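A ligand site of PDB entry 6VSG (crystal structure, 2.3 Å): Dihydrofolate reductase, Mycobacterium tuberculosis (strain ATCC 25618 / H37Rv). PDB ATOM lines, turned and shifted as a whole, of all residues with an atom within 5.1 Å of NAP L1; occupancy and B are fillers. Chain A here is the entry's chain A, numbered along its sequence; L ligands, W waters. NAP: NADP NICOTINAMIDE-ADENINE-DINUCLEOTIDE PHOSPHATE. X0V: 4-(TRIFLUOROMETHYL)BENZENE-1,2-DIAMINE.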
ATOM      1  N   ILE A   7      24.076 -12.436 -13.111  1.00  0.00           N
ATOM      2  CA  ILE A   7      22.633 -12.436 -13.257  1.00  0.00           C
ATOM      3  C   ILE A   7      22.299 -12.089 -14.698  1.00  0.00           C
ATOM      4  O   ILE A   7      22.819 -11.107 -15.248  1.00  0.00           O
ATOM      5  CB  ILE A   7      21.953 -11.461 -12.260  1.00  0.00           C
ATOM      6  CG1 ILE A   7      20.432 -11.509 -12.391  1.00  0.00           C
ATOM      7  CG2 ILE A   7      22.480 -10.048 -12.403  1.00  0.00           C
ATOM      8  CD1 ILE A   7      19.697 -10.981 -11.176  1.00  0.00           C
ATOM      9  N   TRP A   8      21.502 -12.940 -15.338  1.00  0.00           N
ATOM     10  CA  TRP A   8      21.129 -12.687 -16.715  1.00  0.00           C
ATOM     11  C   TRP A   8      19.814 -13.381 -17.014  1.00  0.00           C
ATOM     12  O   TRP A   8      19.360 -14.258 -16.275  1.00  0.00           O
ATOM     13  CB  TRP A   8      22.217 -13.153 -17.690  1.00  0.00           C
ATOM     14  CG  TRP A   8      22.340 -14.631 -17.882  1.00  0.00           C
ATOM     15  CD1 TRP A   8      21.549 -15.421 -18.659  1.00  0.00           C
ATOM     16  CD2 TRP A   8      23.361 -15.493 -17.342  1.00  0.00           C
ATOM     17  NE1 TRP A   8      21.990 -16.721 -18.613  1.00  0.00           N
ATOM     18  CE2 TRP A   8      23.102 -16.792 -17.825  1.00  0.00           C
ATOM     19  CE3 TRP A   8      24.456 -15.286 -16.506  1.00  0.00           C
ATOM     20  CZ2 TRP A   8      23.891 -17.887 -17.490  1.00  0.00           C
ATOM     21  CZ3 TRP A   8      25.246 -16.371 -16.169  1.00  0.00           C
ATOM     22  CH2 TRP A   8      24.960 -17.656 -16.659  1.00  0.00           C
ATOM     23  N   ALA A   9      19.207 -12.976 -18.126  1.00  0.00           N
ATOM     24  CA  ALA A   9      18.018 -13.582 -18.674  1.00  0.00           C
ATOM     25  C   ALA A   9      18.342 -14.076 -20.078  1.00  0.00           C
ATOM     26  O   ALA A   9      18.922 -13.341 -20.872  1.00  0.00           O
ATOM     27  CB  ALA A   9      16.859 -12.587 -18.717  1.00  0.00           C
ATOM     28  N   ILE A  16      21.254 -13.560 -25.123  1.00  0.00           N
ATOM     29  CA  ILE A  16      20.928 -12.588 -24.095  1.00  0.00           C
ATOM     30  C   ILE A  16      20.821 -11.163 -24.619  1.00  0.00           C
ATOM     31  O   ILE A  16      20.147 -10.328 -23.997  1.00  0.00           O
ATOM     32  CB  ILE A  16      21.950 -12.636 -22.933  1.00  0.00           C
ATOM     33  CG1 ILE A  16      23.351 -12.298 -23.437  1.00  0.00           C
ATOM     34  CG2 ILE A  16      21.918 -14.001 -22.267  1.00  0.00           C
ATOM     35  CD1 ILE A  16      24.345 -12.096 -22.324  1.00  0.00           C
ATOM     36  N   GLY A  17      21.456 -10.839 -25.746  1.00  0.00           N
ATOM     37  CA  GLY A  17      21.335  -9.517 -26.307  1.00  0.00           C
ATOM     38  C   GLY A  17      21.468  -9.561 -27.816  1.00  0.00           C
ATOM     39  O   GLY A  17      22.040 -10.494 -28.378  1.00  0.00           O
ATOM     40  N   ARG A  18      20.912  -8.544 -28.469  1.00  0.00           N
ATOM     41  CA  ARG A  18      21.016  -8.426 -29.914  1.00  0.00           C
ATOM     42  C   ARG A  18      20.718  -6.979 -30.290  1.00  0.00           C
ATOM     43  O   ARG A  18      19.748  -6.401 -29.793  1.00  0.00           O
ATOM     44  CB  ARG A  18      20.049  -9.395 -30.611  1.00  0.00           C
ATOM     45  CG  ARG A  18      19.900  -9.171 -32.113  1.00  0.00           C
ATOM     46  CD  ARG A  18      18.871 -10.125 -32.723  1.00  0.00           C
ATOM     47  NE  ARG A  18      19.265 -11.520 -32.561  1.00  0.00           N
ATOM     48  CZ  ARG A  18      18.444 -12.535 -32.793  1.00  0.00           C
ATOM     49  NH1 ARG A  18      17.188 -12.328 -33.184  1.00  0.00           N
ATOM     50  NH2 ARG A  18      18.874 -13.779 -32.631  1.00  0.00           N
ATOM     51  N   GLY A  19      21.585  -6.393 -31.109  1.00  0.00           N
ATOM     52  CA  GLY A  19      21.407  -5.000 -31.514  1.00  0.00           C
ATOM     53  C   GLY A  19      21.548  -3.993 -30.393  1.00  0.00           C
ATOM     54  O   GLY A  19      20.939  -2.922 -30.464  1.00  0.00           O
ATOM     55  N   GLY A  20      22.334  -4.298 -29.376  1.00  0.00           N
ATOM     56  CA  GLY A  20      22.416  -3.414 -28.237  1.00  0.00           C
ATOM     57  C   GLY A  20      21.174  -3.400 -27.392  1.00  0.00           C
ATOM     58  O   GLY A  20      20.938  -2.451 -26.651  1.00  0.00           O
ATOM     59  N   ASP A  21      20.358  -4.450 -27.477  1.00  0.00           N
ATOM     60  CA  ASP A  21      19.066  -4.492 -26.816  1.00  0.00           C
ATOM     61  C   ASP A  21      18.802  -5.939 -26.433  1.00  0.00           C
ATOM     62  O   ASP A  21      19.543  -6.857 -26.804  1.00  0.00           O
ATOM     63  CB  ASP A  21      17.960  -3.958 -27.738  1.00  0.00           C
ATOM     64  CG  ASP A  21      16.684  -3.678 -27.007  1.00  0.00           C
ATOM     65  OD1 ASP A  21      15.656  -4.282 -27.349  1.00  0.00           O
ATOM     66  OD2 ASP A  21      16.705  -2.844 -26.077  1.00  0.00           O
ATOM     67  N   ILE A  22      17.730  -6.125 -25.670  1.00  0.00           N
ATOM     68  CA  ILE A  22      17.222  -7.458 -25.338  1.00  0.00           C
ATOM     69  C   ILE A  22      15.965  -7.676 -26.121  1.00  0.00           C
ATOM     70  O   ILE A  22      15.014  -6.865 -26.019  1.00  0.00           O
ATOM     71  CB  ILE A  22      16.998  -7.616 -23.818  1.00  0.00           C
ATOM     72  CG1 ILE A  22      18.307  -7.364 -23.073  1.00  0.00           C
ATOM     73  CG2 ILE A  22      16.487  -9.011 -23.533  1.00  0.00           C
ATOM     74  CD1 ILE A  22      18.152  -7.054 -21.596  1.00  0.00           C
ATOM     75  N   TRP A  24      13.170  -9.106 -25.994  1.00  0.00           N
ATOM     76  CA  TRP A  24      11.930  -9.473 -25.323  1.00  0.00           C
ATOM     77  C   TRP A  24      11.755  -8.540 -24.133  1.00  0.00           C
ATOM     78  O   TRP A  24      12.632  -7.733 -23.821  1.00  0.00           O
ATOM     79  CB  TRP A  24      11.935 -10.942 -24.892  1.00  0.00           C
ATOM     80  CG  TRP A  24      12.905 -11.224 -23.809  1.00  0.00           C
ATOM     81  CD1 TRP A  24      12.726 -10.992 -22.476  1.00  0.00           C
ATOM     82  CD2 TRP A  24      14.226 -11.767 -23.951  1.00  0.00           C
ATOM     83  NE1 TRP A  24      13.848 -11.361 -21.788  1.00  0.00           N
ATOM     84  CE2 TRP A  24      14.783 -11.826 -22.670  1.00  0.00           C
ATOM     85  CE3 TRP A  24      14.979 -12.189 -25.050  1.00  0.00           C
ATOM     86  CZ2 TRP A  24      16.074 -12.318 -22.442  1.00  0.00           C
ATOM     87  CZ3 TRP A  24      16.270 -12.680 -24.822  1.00  0.00           C
ATOM     88  CH2 TRP A  24      16.798 -12.733 -23.518  1.00  0.00           C
ATOM     89  N   GLY A  45      29.704  -4.337 -18.661  1.00  0.00           N
ATOM     90  CA  GLY A  45      30.504  -3.895 -19.776  1.00  0.00           C
ATOM     91  C   GLY A  45      30.026  -2.586 -20.339  1.00  0.00           C
ATOM     92  O   GLY A  45      28.875  -2.172 -20.187  1.00  0.00           O
ATOM     93  N   ARG A  46      30.953  -1.914 -21.019  1.00  0.00           N
ATOM     94  CA  ARG A  46      30.694  -0.562 -21.486  1.00  0.00           C
ATOM     95  C   ARG A  46      29.560  -0.550 -22.502  1.00  0.00           C
ATOM     96  O   ARG A  46      28.765   0.402 -22.529  1.00  0.00           O
ATOM     97  CB  ARG A  46      31.995   0.029 -22.077  1.00  0.00           C
ATOM     98  CG  ARG A  46      32.002   1.526 -22.411  1.00  0.00           C
ATOM     99  CD  ARG A  46      31.310   1.806 -23.756  1.00  0.00           C
ATOM    100  NE  ARG A  46      32.138   1.183 -24.767  1.00  0.00           N
ATOM    101  CZ  ARG A  46      31.726   0.878 -25.986  1.00  0.00           C
ATOM    102  NH1 ARG A  46      30.480   1.118 -26.389  1.00  0.00           N
ATOM    103  NH2 ARG A  46      32.584   0.304 -26.822  1.00  0.00           N
ATOM    104  N   ARG A  47      29.465  -1.583 -23.348  1.00  0.00           N
ATOM    105  CA  ARG A  47      28.313  -1.697 -24.254  1.00  0.00           C
ATOM    106  C   ARG A  47      27.008  -1.784 -23.487  1.00  0.00           C
ATOM    107  O   ARG A  47      26.037  -1.102 -23.801  1.00  0.00           O
ATOM    108  CB  ARG A  47      28.463  -2.908 -25.170  1.00  0.00           C
ATOM    109  CG  ARG A  47      29.685  -2.904 -26.041  1.00  0.00           C
ATOM    110  CD  ARG A  47      29.426  -3.620 -27.359  1.00  0.00           C
ATOM    111  NE  ARG A  47      30.638  -3.671 -28.169  1.00  0.00           N
ATOM    112  CZ  ARG A  47      31.109  -4.780 -28.739  1.00  0.00           C
ATOM    113  NH1 ARG A  47      30.459  -5.932 -28.615  1.00  0.00           N
ATOM    114  NH2 ARG A  47      32.235  -4.725 -29.442  1.00  0.00           N
ATOM    115  N   THR A  48      26.959  -2.653 -22.466  1.00  0.00           N
ATOM    116  CA  THR A  48      25.748  -2.735 -21.660  1.00  0.00           C
ATOM    117  C   THR A  48      25.418  -1.396 -21.020  1.00  0.00           C
ATOM    118  O   THR A  48      24.248  -0.992 -20.999  1.00  0.00           O
ATOM    119  CB  THR A  48      25.884  -3.834 -20.600  1.00  0.00           C
ATOM    120  OG1 THR A  48      25.892  -5.116 -21.247  1.00  0.00           O
ATOM    121  CG2 THR A  48      24.725  -3.783 -19.671  1.00  0.00           C
ATOM    122  N   SER A  51      23.682   0.711 -23.334  1.00  0.00           N
ATOM    123  CA  SER A  51      22.342   0.234 -23.676  1.00  0.00           C
ATOM    124  C   SER A  51      21.268   0.804 -22.752  1.00  0.00           C
ATOM    125  O   SER A  51      20.090   0.848 -23.133  1.00  0.00           O
ATOM    126  CB  SER A  51      22.289  -1.283 -23.639  1.00  0.00           C
ATOM    127  OG  SER A  51      22.408  -1.771 -22.321  1.00  0.00           O
ATOM    128  N   LEU A  67      33.089  -1.505 -16.983  1.00  0.00           N
ATOM    129  CA  LEU A  67      34.376  -2.065 -17.394  1.00  0.00           C
ATOM    130  C   LEU A  67      34.675  -1.673 -18.839  1.00  0.00           C
ATOM    131  O   LEU A  67      33.864  -1.919 -19.735  1.00  0.00           O
ATOM    132  CB  LEU A  67      34.322  -3.589 -17.239  1.00  0.00           C
ATOM    133  CG  LEU A  67      35.566  -4.419 -17.535  1.00  0.00           C
ATOM    134  CD1 LEU A  67      36.726  -3.999 -16.663  1.00  0.00           C
ATOM    135  CD2 LEU A  67      35.239  -5.876 -17.310  1.00  0.00           C
ATOM    136  N   SER A  68      35.828  -1.041 -19.065  1.00  0.00           N
ATOM    137  CA  SER A  68      36.186  -0.585 -20.407  1.00  0.00           C
ATOM    138  C   SER A  68      37.691  -0.582 -20.609  1.00  0.00           C
ATOM    139  O   SER A  68      38.465  -0.482 -19.647  1.00  0.00           O
ATOM    140  CB  SER A  68      35.644   0.829 -20.690  1.00  0.00           C
ATOM    141  OG  SER A  68      36.146   1.309 -21.916  1.00  0.00           O
ATOM    142  N   ARG A  69      38.099  -0.713 -21.874  1.00  0.00           N
ATOM    143  CA  ARG A  69      39.507  -0.605 -22.235  1.00  0.00           C
ATOM    144  C   ARG A  69      39.911   0.829 -22.565  1.00  0.00           C
ATOM    145  O   ARG A  69      41.103   1.127 -22.602  1.00  0.00           O
ATOM    146  CB  ARG A  69      39.823  -1.495 -23.436  1.00  0.00           C
ATOM    147  CG  ARG A  69      39.521  -2.961 -23.225  1.00  0.00           C
ATOM    148  CD  ARG A  69      40.123  -3.786 -24.354  1.00  0.00           C
ATOM    149  NE  ARG A  69      40.621  -5.069 -23.866  1.00  0.00           N
ATOM    150  CZ  ARG A  69      39.926  -6.207 -23.877  1.00  0.00           C
ATOM    151  NH1 ARG A  69      38.702  -6.217 -24.364  1.00  0.00           N
ATOM    152  NH2 ARG A  69      40.467  -7.325 -23.404  1.00  0.00           N
ATOM    153  N   GLN A  70      38.943   1.705 -22.828  1.00  0.00           N
ATOM    154  CA  GLN A  70      39.234   3.107 -23.068  1.00  0.00           C
ATOM    155  C   GLN A  70      39.893   3.708 -21.833  1.00  0.00           C
ATOM    156  O   GLN A  70      39.403   3.530 -20.717  1.00  0.00           O
ATOM    157  CB  GLN A  70      37.957   3.863 -23.423  1.00  0.00           C
ATOM    158  CG  GLN A  70      37.385   3.424 -24.766  1.00  0.00           C
ATOM    159  CD  GLN A  70      36.079   4.116 -25.102  1.00  0.00           C
ATOM    160  OE1 GLN A  70      36.036   5.341 -25.268  1.00  0.00           O
ATOM    161  NE2 GLN A  70      35.004   3.339 -25.212  1.00  0.00           N
ATOM    162  N   PHE A  73      37.722   6.631 -20.348  1.00  0.00           N
ATOM    163  CA  PHE A  73      36.288   6.548 -20.583  1.00  0.00           C
ATOM    164  C   PHE A  73      35.540   7.076 -19.363  1.00  0.00           C
ATOM    165  O   PHE A  73      35.850   6.707 -18.220  1.00  0.00           O
ATOM    166  CB  PHE A  73      35.844   5.127 -20.879  1.00  0.00           C
ATOM    167  CG  PHE A  73      34.370   5.009 -21.170  1.00  0.00           C
ATOM    168  CD1 PHE A  73      33.468   4.745 -20.169  1.00  0.00           C
ATOM    169  CD2 PHE A  73      33.888   5.207 -22.448  1.00  0.00           C
ATOM    170  CE1 PHE A  73      32.107   4.663 -20.429  1.00  0.00           C
ATOM    171  CE2 PHE A  73      32.540   5.115 -22.717  1.00  0.00           C
ATOM    172  CZ  PHE A  73      31.643   4.848 -21.703  1.00  0.00           C
ATOM    173  N   VAL A  81      36.523   1.206 -14.577  1.00  0.00           N
ATOM    174  CA  VAL A  81      37.727   0.459 -14.281  1.00  0.00           C
ATOM    175  C   VAL A  81      38.194  -0.252 -15.551  1.00  0.00           C
ATOM    176  O   VAL A  81      37.425  -0.436 -16.505  1.00  0.00           O
ATOM    177  CB  VAL A  81      37.506  -0.556 -13.149  1.00  0.00           C
ATOM    178  CG1 VAL A  81      36.977   0.160 -11.881  1.00  0.00           C
ATOM    179  CG2 VAL A  81      36.549  -1.654 -13.606  1.00  0.00           C
ATOM    180  N   GLY A  82      39.456  -0.646 -15.556  1.00  0.00           N
ATOM    181  CA  GLY A  82      40.061  -1.200 -16.751  1.00  0.00           C
ATOM    182  C   GLY A  82      40.218  -2.707 -16.694  1.00  0.00           C
ATOM    183  O   GLY A  82      40.457  -3.352 -17.724  1.00  0.00           O
ATOM    184  N   SER A  83      40.094  -3.268 -15.509  1.00  0.00           N
ATOM    185  CA  SER A  83      40.110  -4.710 -15.332  1.00  0.00           C
ATOM    186  C   SER A  83      38.952  -5.097 -14.424  1.00  0.00           C
ATOM    187  O   SER A  83      38.560  -4.334 -13.541  1.00  0.00           O
ATOM    188  CB  SER A  83      41.430  -5.204 -14.743  1.00  0.00           C
ATOM    189  OG  SER A  83      41.587  -4.752 -13.408  1.00  0.00           O
ATOM    190  N   ILE A  96      26.264  -7.795 -14.380  1.00  0.00           N
ATOM    191  CA  ILE A  96      24.972  -7.703 -15.017  1.00  0.00           C
ATOM    192  C   ILE A  96      25.079  -7.689 -16.547  1.00  0.00           C
ATOM    193  O   ILE A  96      24.156  -7.257 -17.220  1.00  0.00           O
ATOM    194  CB  ILE A  96      24.179  -6.481 -14.518  1.00  0.00           C
ATOM    195  CG1 ILE A  96      24.863  -5.179 -14.906  1.00  0.00           C
ATOM    196  CG2 ILE A  96      23.996  -6.575 -13.023  1.00  0.00           C
ATOM    197  CD1 ILE A  96      23.958  -3.965 -14.781  1.00  0.00           C
ATOM    198  N   GLY A  97      26.193  -8.172 -17.099  1.00  0.00           N
ATOM    199  CA  GLY A  97      26.359  -8.255 -18.538  1.00  0.00           C
ATOM    200  C   GLY A  97      27.412  -7.311 -19.059  1.00  0.00           C
ATOM    201  O   GLY A  97      27.978  -6.551 -18.299  1.00  0.00           O
ATOM    202  N   GLY A  98      27.684  -7.361 -20.361  1.00  0.00           N
ATOM    203  CA  GLY A  98      26.992  -8.241 -21.271  1.00  0.00           C
ATOM    204  C   GLY A  98      27.697  -9.563 -21.485  1.00  0.00           C
ATOM    205  O   GLY A  98      28.392 -10.057 -20.597  1.00  0.00           O
ATOM    206  N   GLY A  99      27.500 -10.128 -22.672  1.00  0.00           N
ATOM    207  CA  GLY A  99      28.088 -11.417 -22.992  1.00  0.00           C
ATOM    208  C   GLY A  99      29.580 -11.442 -22.755  1.00  0.00           C
ATOM    209  O   GLY A  99      30.116 -12.391 -22.163  1.00  0.00           O
ATOM    210  N   GLN A 100      30.291 -10.400 -23.184  1.00  0.00           N
ATOM    211  CA  GLN A 100      31.740 -10.382 -22.989  1.00  0.00           C
ATOM    212  C   GLN A 100      32.094 -10.370 -21.501  1.00  0.00           C
ATOM    213  O   GLN A 100      33.045 -11.046 -21.072  1.00  0.00           O
ATOM    214  CB  GLN A 100      32.348  -9.169 -23.676  1.00  0.00           C
ATOM    215  CG  GLN A 100      32.509  -9.298 -25.181  1.00  0.00           C
ATOM    216  CD  GLN A 100      33.119  -8.046 -25.772  1.00  0.00           C
ATOM    217  OE1 GLN A 100      34.056  -7.463 -25.219  1.00  0.00           O
ATOM    218  NE2 GLN A 100      32.556  -7.591 -26.889  1.00  0.00           N
ATOM    219  N   VAL A 101      31.336  -9.634 -20.691  1.00  0.00           N
ATOM    220  CA  VAL A 101      31.714  -9.505 -19.279  1.00  0.00           C
ATOM    221  C   VAL A 101      31.268 -10.716 -18.472  1.00  0.00           C
ATOM    222  O   VAL A 101      31.972 -11.128 -17.543  1.00  0.00           O
ATOM    223  CB  VAL A 101      31.201  -8.168 -18.701  1.00  0.00           C
ATOM    224  CG1 VAL A 101      31.564  -8.043 -17.219  1.00  0.00           C
ATOM    225  CG2 VAL A 101      31.856  -7.012 -19.425  1.00  0.00           C
ATOM    226  N   TYR A 102      30.119 -11.332 -18.810  1.00  0.00           N
ATOM    227  CA  TYR A 102      29.769 -12.604 -18.174  1.00  0.00           C
ATOM    228  C   TYR A 102      30.871 -13.622 -18.368  1.00  0.00           C
ATOM    229  O   TYR A 102      31.278 -14.303 -17.423  1.00  0.00           O
ATOM    230  CB  TYR A 102      28.456 -13.170 -18.720  1.00  0.00           C
ATOM    231  CG  TYR A 102      27.212 -12.420 -18.342  1.00  0.00           C
ATOM    232  CD1 TYR A 102      26.968 -12.025 -17.025  1.00  0.00           C
ATOM    233  CD2 TYR A 102      26.250 -12.145 -19.303  1.00  0.00           C
ATOM    234  CE1 TYR A 102      25.807 -11.351 -16.705  1.00  0.00           C
ATOM    235  CE2 TYR A 102      25.103 -11.471 -18.989  1.00  0.00           C
ATOM    236  CZ  TYR A 102      24.888 -11.074 -17.693  1.00  0.00           C
ATOM    237  OH  TYR A 102      23.729 -10.393 -17.403  1.00  0.00           O
ATOM    238  N   LEU A 104      34.065 -13.144 -19.096  1.00  0.00           N
ATOM    239  CA  LEU A 104      35.255 -12.759 -18.350  1.00  0.00           C
ATOM    240  C   LEU A 104      35.078 -12.998 -16.849  1.00  0.00           C
ATOM    241  O   LEU A 104      36.053 -13.335 -16.157  1.00  0.00           O
ATOM    242  CB  LEU A 104      35.556 -11.281 -18.614  1.00  0.00           C
ATOM    243  CG  LEU A 104      36.679 -10.612 -17.827  1.00  0.00           C
ATOM    244  CD1 LEU A 104      38.016 -11.234 -18.165  1.00  0.00           C
ATOM    245  CD2 LEU A 104      36.694  -9.102 -18.088  1.00  0.00           C
ATOM    246  N   ALA A 128      24.834 -11.470 -28.559  1.00  0.00           N
ATOM    247  CA  ALA A 128      25.441 -11.712 -27.262  1.00  0.00           C
ATOM    248  C   ALA A 128      24.830 -12.974 -26.673  1.00  0.00           C
ATOM    249  O   ALA A 128      23.614 -13.185 -26.738  1.00  0.00           O
ATOM    250  CB  ALA A 128      25.211 -10.518 -26.338  1.00  0.00           C
HETATM  251  PA  NAP L   1      29.451  -5.958 -23.024  1.00  0.00           P
HETATM  252  O1A NAP L   1      30.055  -7.271 -22.663  1.00  0.00           O
HETATM  253  O2A NAP L   1      28.196  -5.446 -22.369  1.00  0.00           O
HETATM  254  O5B NAP L   1      30.597  -4.846 -22.785  1.00  0.00           O
HETATM  255  C5B NAP L   1      31.486  -4.990 -23.840  1.00  0.00           C
HETATM  256  C4B NAP L   1      32.608  -4.045 -23.491  1.00  0.00           C
HETATM  257  O4B NAP L   1      33.157  -4.458 -22.283  1.00  0.00           O
HETATM  258  C3B NAP L   1      33.735  -4.032 -24.507  1.00  0.00           C
HETATM  259  O3B NAP L   1      33.391  -3.209 -25.595  1.00  0.00           O
HETATM  260  C2B NAP L   1      34.738  -3.262 -23.671  1.00  0.00           C
HETATM  261  O2B NAP L   1      34.415  -1.995 -23.525  1.00  0.00           O
HETATM  262  C1B NAP L   1      34.466  -3.914 -22.268  1.00  0.00           C
HETATM  263  N9A NAP L   1      35.379  -4.990 -21.968  1.00  0.00           N
HETATM  264  C8A NAP L   1      35.334  -6.326 -22.406  1.00  0.00           C
HETATM  265  N7A NAP L   1      36.355  -7.060 -21.929  1.00  0.00           N
HETATM  266  C5A NAP L   1      37.089  -6.153 -21.150  1.00  0.00           C
HETATM  267  C6A NAP L   1      38.266  -6.294 -20.395  1.00  0.00           C
HETATM  268  N6A NAP L   1      38.889  -7.508 -20.335  1.00  0.00           N
HETATM  269  N1A NAP L   1      38.805  -5.251 -19.699  1.00  0.00           N
HETATM  270  C2A NAP L   1      38.125  -4.059 -19.818  1.00  0.00           C
HETATM  271  N3A NAP L   1      37.006  -3.768 -20.488  1.00  0.00           N
HETATM  272  C4A NAP L   1      36.494  -4.860 -21.161  1.00  0.00           C
HETATM  273  O3  NAP L   1      29.214  -6.025 -24.707  1.00  0.00           O
HETATM  274  PN  NAP L   1      28.393  -7.327 -25.216  1.00  0.00           P
HETATM  275  O1N NAP L   1      27.915  -7.047 -26.586  1.00  0.00           O
HETATM  276  O2N NAP L   1      28.996  -8.669 -24.862  1.00  0.00           O
HETATM  277  O5D NAP L   1      26.843  -7.386 -24.354  1.00  0.00           O
HETATM  278  C5D NAP L   1      26.013  -6.383 -24.855  1.00  0.00           C
HETATM  279  C4D NAP L   1      24.634  -7.001 -25.065  1.00  0.00           C
HETATM  280  O4D NAP L   1      24.246  -7.718 -23.874  1.00  0.00           O
HETATM  281  C3D NAP L   1      23.557  -5.903 -25.317  1.00  0.00           C
HETATM  282  O3D NAP L   1      22.754  -6.347 -26.381  1.00  0.00           O
HETATM  283  C2D NAP L   1      22.782  -5.930 -24.000  1.00  0.00           C
HETATM  284  O2D NAP L   1      21.433  -5.646 -24.160  1.00  0.00           O
HETATM  285  C1D NAP L   1      22.892  -7.426 -23.663  1.00  0.00           C
HETATM  286  N1N NAP L   1      22.622  -7.648 -22.251  1.00  0.00           N
HETATM  287  C2N NAP L   1      21.710  -8.609 -21.885  1.00  0.00           C
HETATM  288  C3N NAP L   1      21.462  -8.870 -20.580  1.00  0.00           C
HETATM  289  C7N NAP L   1      20.502  -9.904 -20.325  1.00  0.00           C
HETATM  290  O7N NAP L   1      19.834 -10.485 -21.198  1.00  0.00           O
HETATM  291  N7N NAP L   1      20.326 -10.253 -19.020  1.00  0.00           N
HETATM  292  C4N NAP L   1      22.135  -8.146 -19.479  1.00  0.00           C
HETATM  293  C5N NAP L   1      23.064  -7.105 -19.975  1.00  0.00           C
HETATM  294  C6N NAP L   1      23.283  -6.893 -21.280  1.00  0.00           C
HETATM  295  P2B NAP L   1      35.391  -0.853 -24.518  1.00  0.00           P
HETATM  296  O1X NAP L   1      34.745  -1.212 -25.830  1.00  0.00           O
HETATM  297  O2X NAP L   1      35.020   0.490 -23.883  1.00  0.00           O
HETATM  298  O3X NAP L   1      36.764  -1.412 -24.249  1.00  0.00           O
HETATM  299  C1  X0V L   2      20.403  -4.968 -17.639  1.00  0.00           C
HETATM  300  C2  X0V L   2      19.369  -3.842 -17.671  1.00  0.00           C
HETATM  301  C3  X0V L   2      17.989  -2.227 -16.538  1.00  0.00           C
HETATM  302  C4  X0V L   2      18.936  -3.248 -16.487  1.00  0.00           C
HETATM  303  C6  X0V L   2      17.463  -1.806 -17.746  1.00  0.00           C
HETATM  304  C7  X0V L   2      18.834  -3.419 -18.882  1.00  0.00           C
HETATM  305  F1  X0V L   2      19.976  -5.984 -18.449  1.00  0.00           F
HETATM  306  F2  X0V L   2      20.516  -5.438 -16.353  1.00  0.00           F
HETATM  307  F3  X0V L   2      21.634  -4.536 -18.049  1.00  0.00           F
HETATM  308  C8  X0V L   2      17.883  -2.400 -18.924  1.00  0.00           C
HETATM  309  N1  X0V L   2      17.540  -1.622 -15.305  1.00  0.00           N
HETATM  310  N2  X0V L   2      16.476  -0.758 -17.764  1.00  0.00           N
HETATM  311  O   HOH W   1      20.653  -3.749 -22.482  1.00  0.00           O
HETATM  312  O   HOH W   2      18.558  -8.192 -17.099  1.00  0.00           O
HETATM  313  O   HOH W   3      39.358  -9.514 -22.508  1.00  0.00           O
HETATM  314  O   HOH W   4      28.792 -10.545 -27.374  1.00  0.00           O
HETATM  315  O   HOH W   5      38.147  -2.315 -26.288  1.00  0.00           O
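The backbone NH (N) of Ser 68 lies close to a nitrogen (N3A) of NAP L1, at 3.3 Å.
The side-chain hydroxyl (OG) of Ser 68 lies within hydrogen-bond range of an oxygen (O2X) of NAP L1, 2.4 Å away.
The backbone NH (N) of Thr 48 lies within hydrogen-bond range of an oxygen (O2A) of NAP L1 (3.1 Å).
OG1 of Thr 48 is in hydrogen-bond range of O2A of NAP L1 (2.6 Å).
The backbone NH (N) of Gln 100 sits at hydrogen-bond distance from an oxygen (O2N) of NAP L1, at 2.7 Å.
An oxygen (O3X) of NAP L1 is in hydrogen-bond range of the backbone NH (N) of Arg 69 (2.8 Å).
The guanidinium group (NH1) of Arg 69 lies within hydrogen-bond range of a nitrogen (N7A) of NAP L1, 3.5 Å away.
The backbone NH (N) of Arg 46 lies within hydrogen-bond range of an oxygen (O5B) of NAP L1, at 3.4 Å.
The guanidinium group (NH2) of Arg 46 is in salt-bridge range of an oxygen (O1X) of NAP L1 (2.8 Å).
The backbone NH (N) of Gly 98 is in hydrogen-bond range of an oxygen (O2A) of NAP L1, 2.8 Å away.
The backbone NH (N) of Gly 99 sits at hydrogen-bond distance from an oxygen (O2N) of NAP L1, 3.0 Å away.
O2X of NAP L1 is in hydrogen-bond range of NE2 of Gln 70 (3.1 Å).
N of Arg 47 sits at hydrogen-bond distance from O5B of NAP L1 (3.5 Å).
The guanidinium group (NH1) of Arg 47 is in salt-bridge range of an oxygen (O1N) of NAP L1, 3.4 Å away.
The backbone NH of Asp 21 is in hydrogen-bond range of an oxygen (O3D) of NAP L1 (3.2 Å).
An oxygen (O3D) of NAP L1 sits at hydrogen-bond distance from the backbone carbonyl oxygen (O) of Asp 21.
N of Val 101 sits at hydrogen-bond distance from O1A of NAP L1 (3.3 Å).
OG of Ser 68 lies within hydrogen-bond range of N of Gln 70 (3.0 Å).
The backbone carbonyl oxygen of Val 81 sits at hydrogen-bond distance from the backbone NH of Ser 68, at 3.1 Å.
OG1 of Thr 48 lies within hydrogen-bond range of N of Gly 98 (3.0 Å).
NE2 of Gln 100 sits close to NH1 of Arg 47 (3.2 Å).
The backbone carbonyl oxygen (O) of Leu 67 sits at hydrogen-bond distance from the backbone NH (N) of Arg 46 (3.2 Å).
O of Gly 97 is in hydrogen-bond range of N of Gly 45, at 2.8 Å.
The side-chain hydroxyl (OH) of Tyr 102 sits close to the backbone NH (N) of Gly 97 (3.3 Å).
The side-chain hydroxyl (OH) of Tyr 102 is in hydrogen-bond range of the backbone carbonyl oxygen (O) of Ile 7 (2.4 Å).
The backbone carbonyl oxygen (O) of Ala 9 lies close to an oxygen (O7N) of NAP L1, at 3.0 Å.
O7N of NAP L1 lies close to O of Ile 16 (2.8 Å).
A nitrogen (N1A) of NAP L1 sits close to the backbone carbonyl oxygen (O) of Gly 82, 3.2 Å away.
Residues that only touch NAP L1: Trp 8 (3.4 Å), Gly 17 (3.5 Å), Arg 18 (3.5 Å), Gly 20 (3.5 Å), Ile 22 (3.7 Å), Gly 45 (3.2 Å), Leu 67 (3.3 Å), Ile 96 (3.0 Å), Gly 97 (3.8 Å), Tyr 102 (3.4 Å), Leu 104 (3.5 Å) and Ala 128 (3.8 Å).
Hydrophobic or aromatic side chains that line NAP L1: Trp 8, Ile 16, Ile 22, Leu 67, Val 101, Leu 104 and Ala 128.
26 residues have an atom within 4 Å of NAP L1: Trp 8, Ala 9, Ile 16, Gly 17, Arg 18, Gly 20, Asp 21, Ile 22, Gly 45, Arg 46, Arg 47, Thr 48, Leu 67, Ser 68, Arg 69, Gln 70, Gly 82, Ile 96, Gly 97, Gly 98, Gly 99, Gln 100, Val 101, Tyr 102, Leu 104 and Ala 128.
Water W1 lies within hydrogen-bond range of an oxygen (O2D) of NAP L1 (2.7 Å) and the side-chain hydroxyl of Ser 51 (2.6 Å).
Water W3 bridges the guanidinium group of Arg 69 (2.6 Å) and a nitrogen (N6A) of NAP L1 (3.0 Å).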
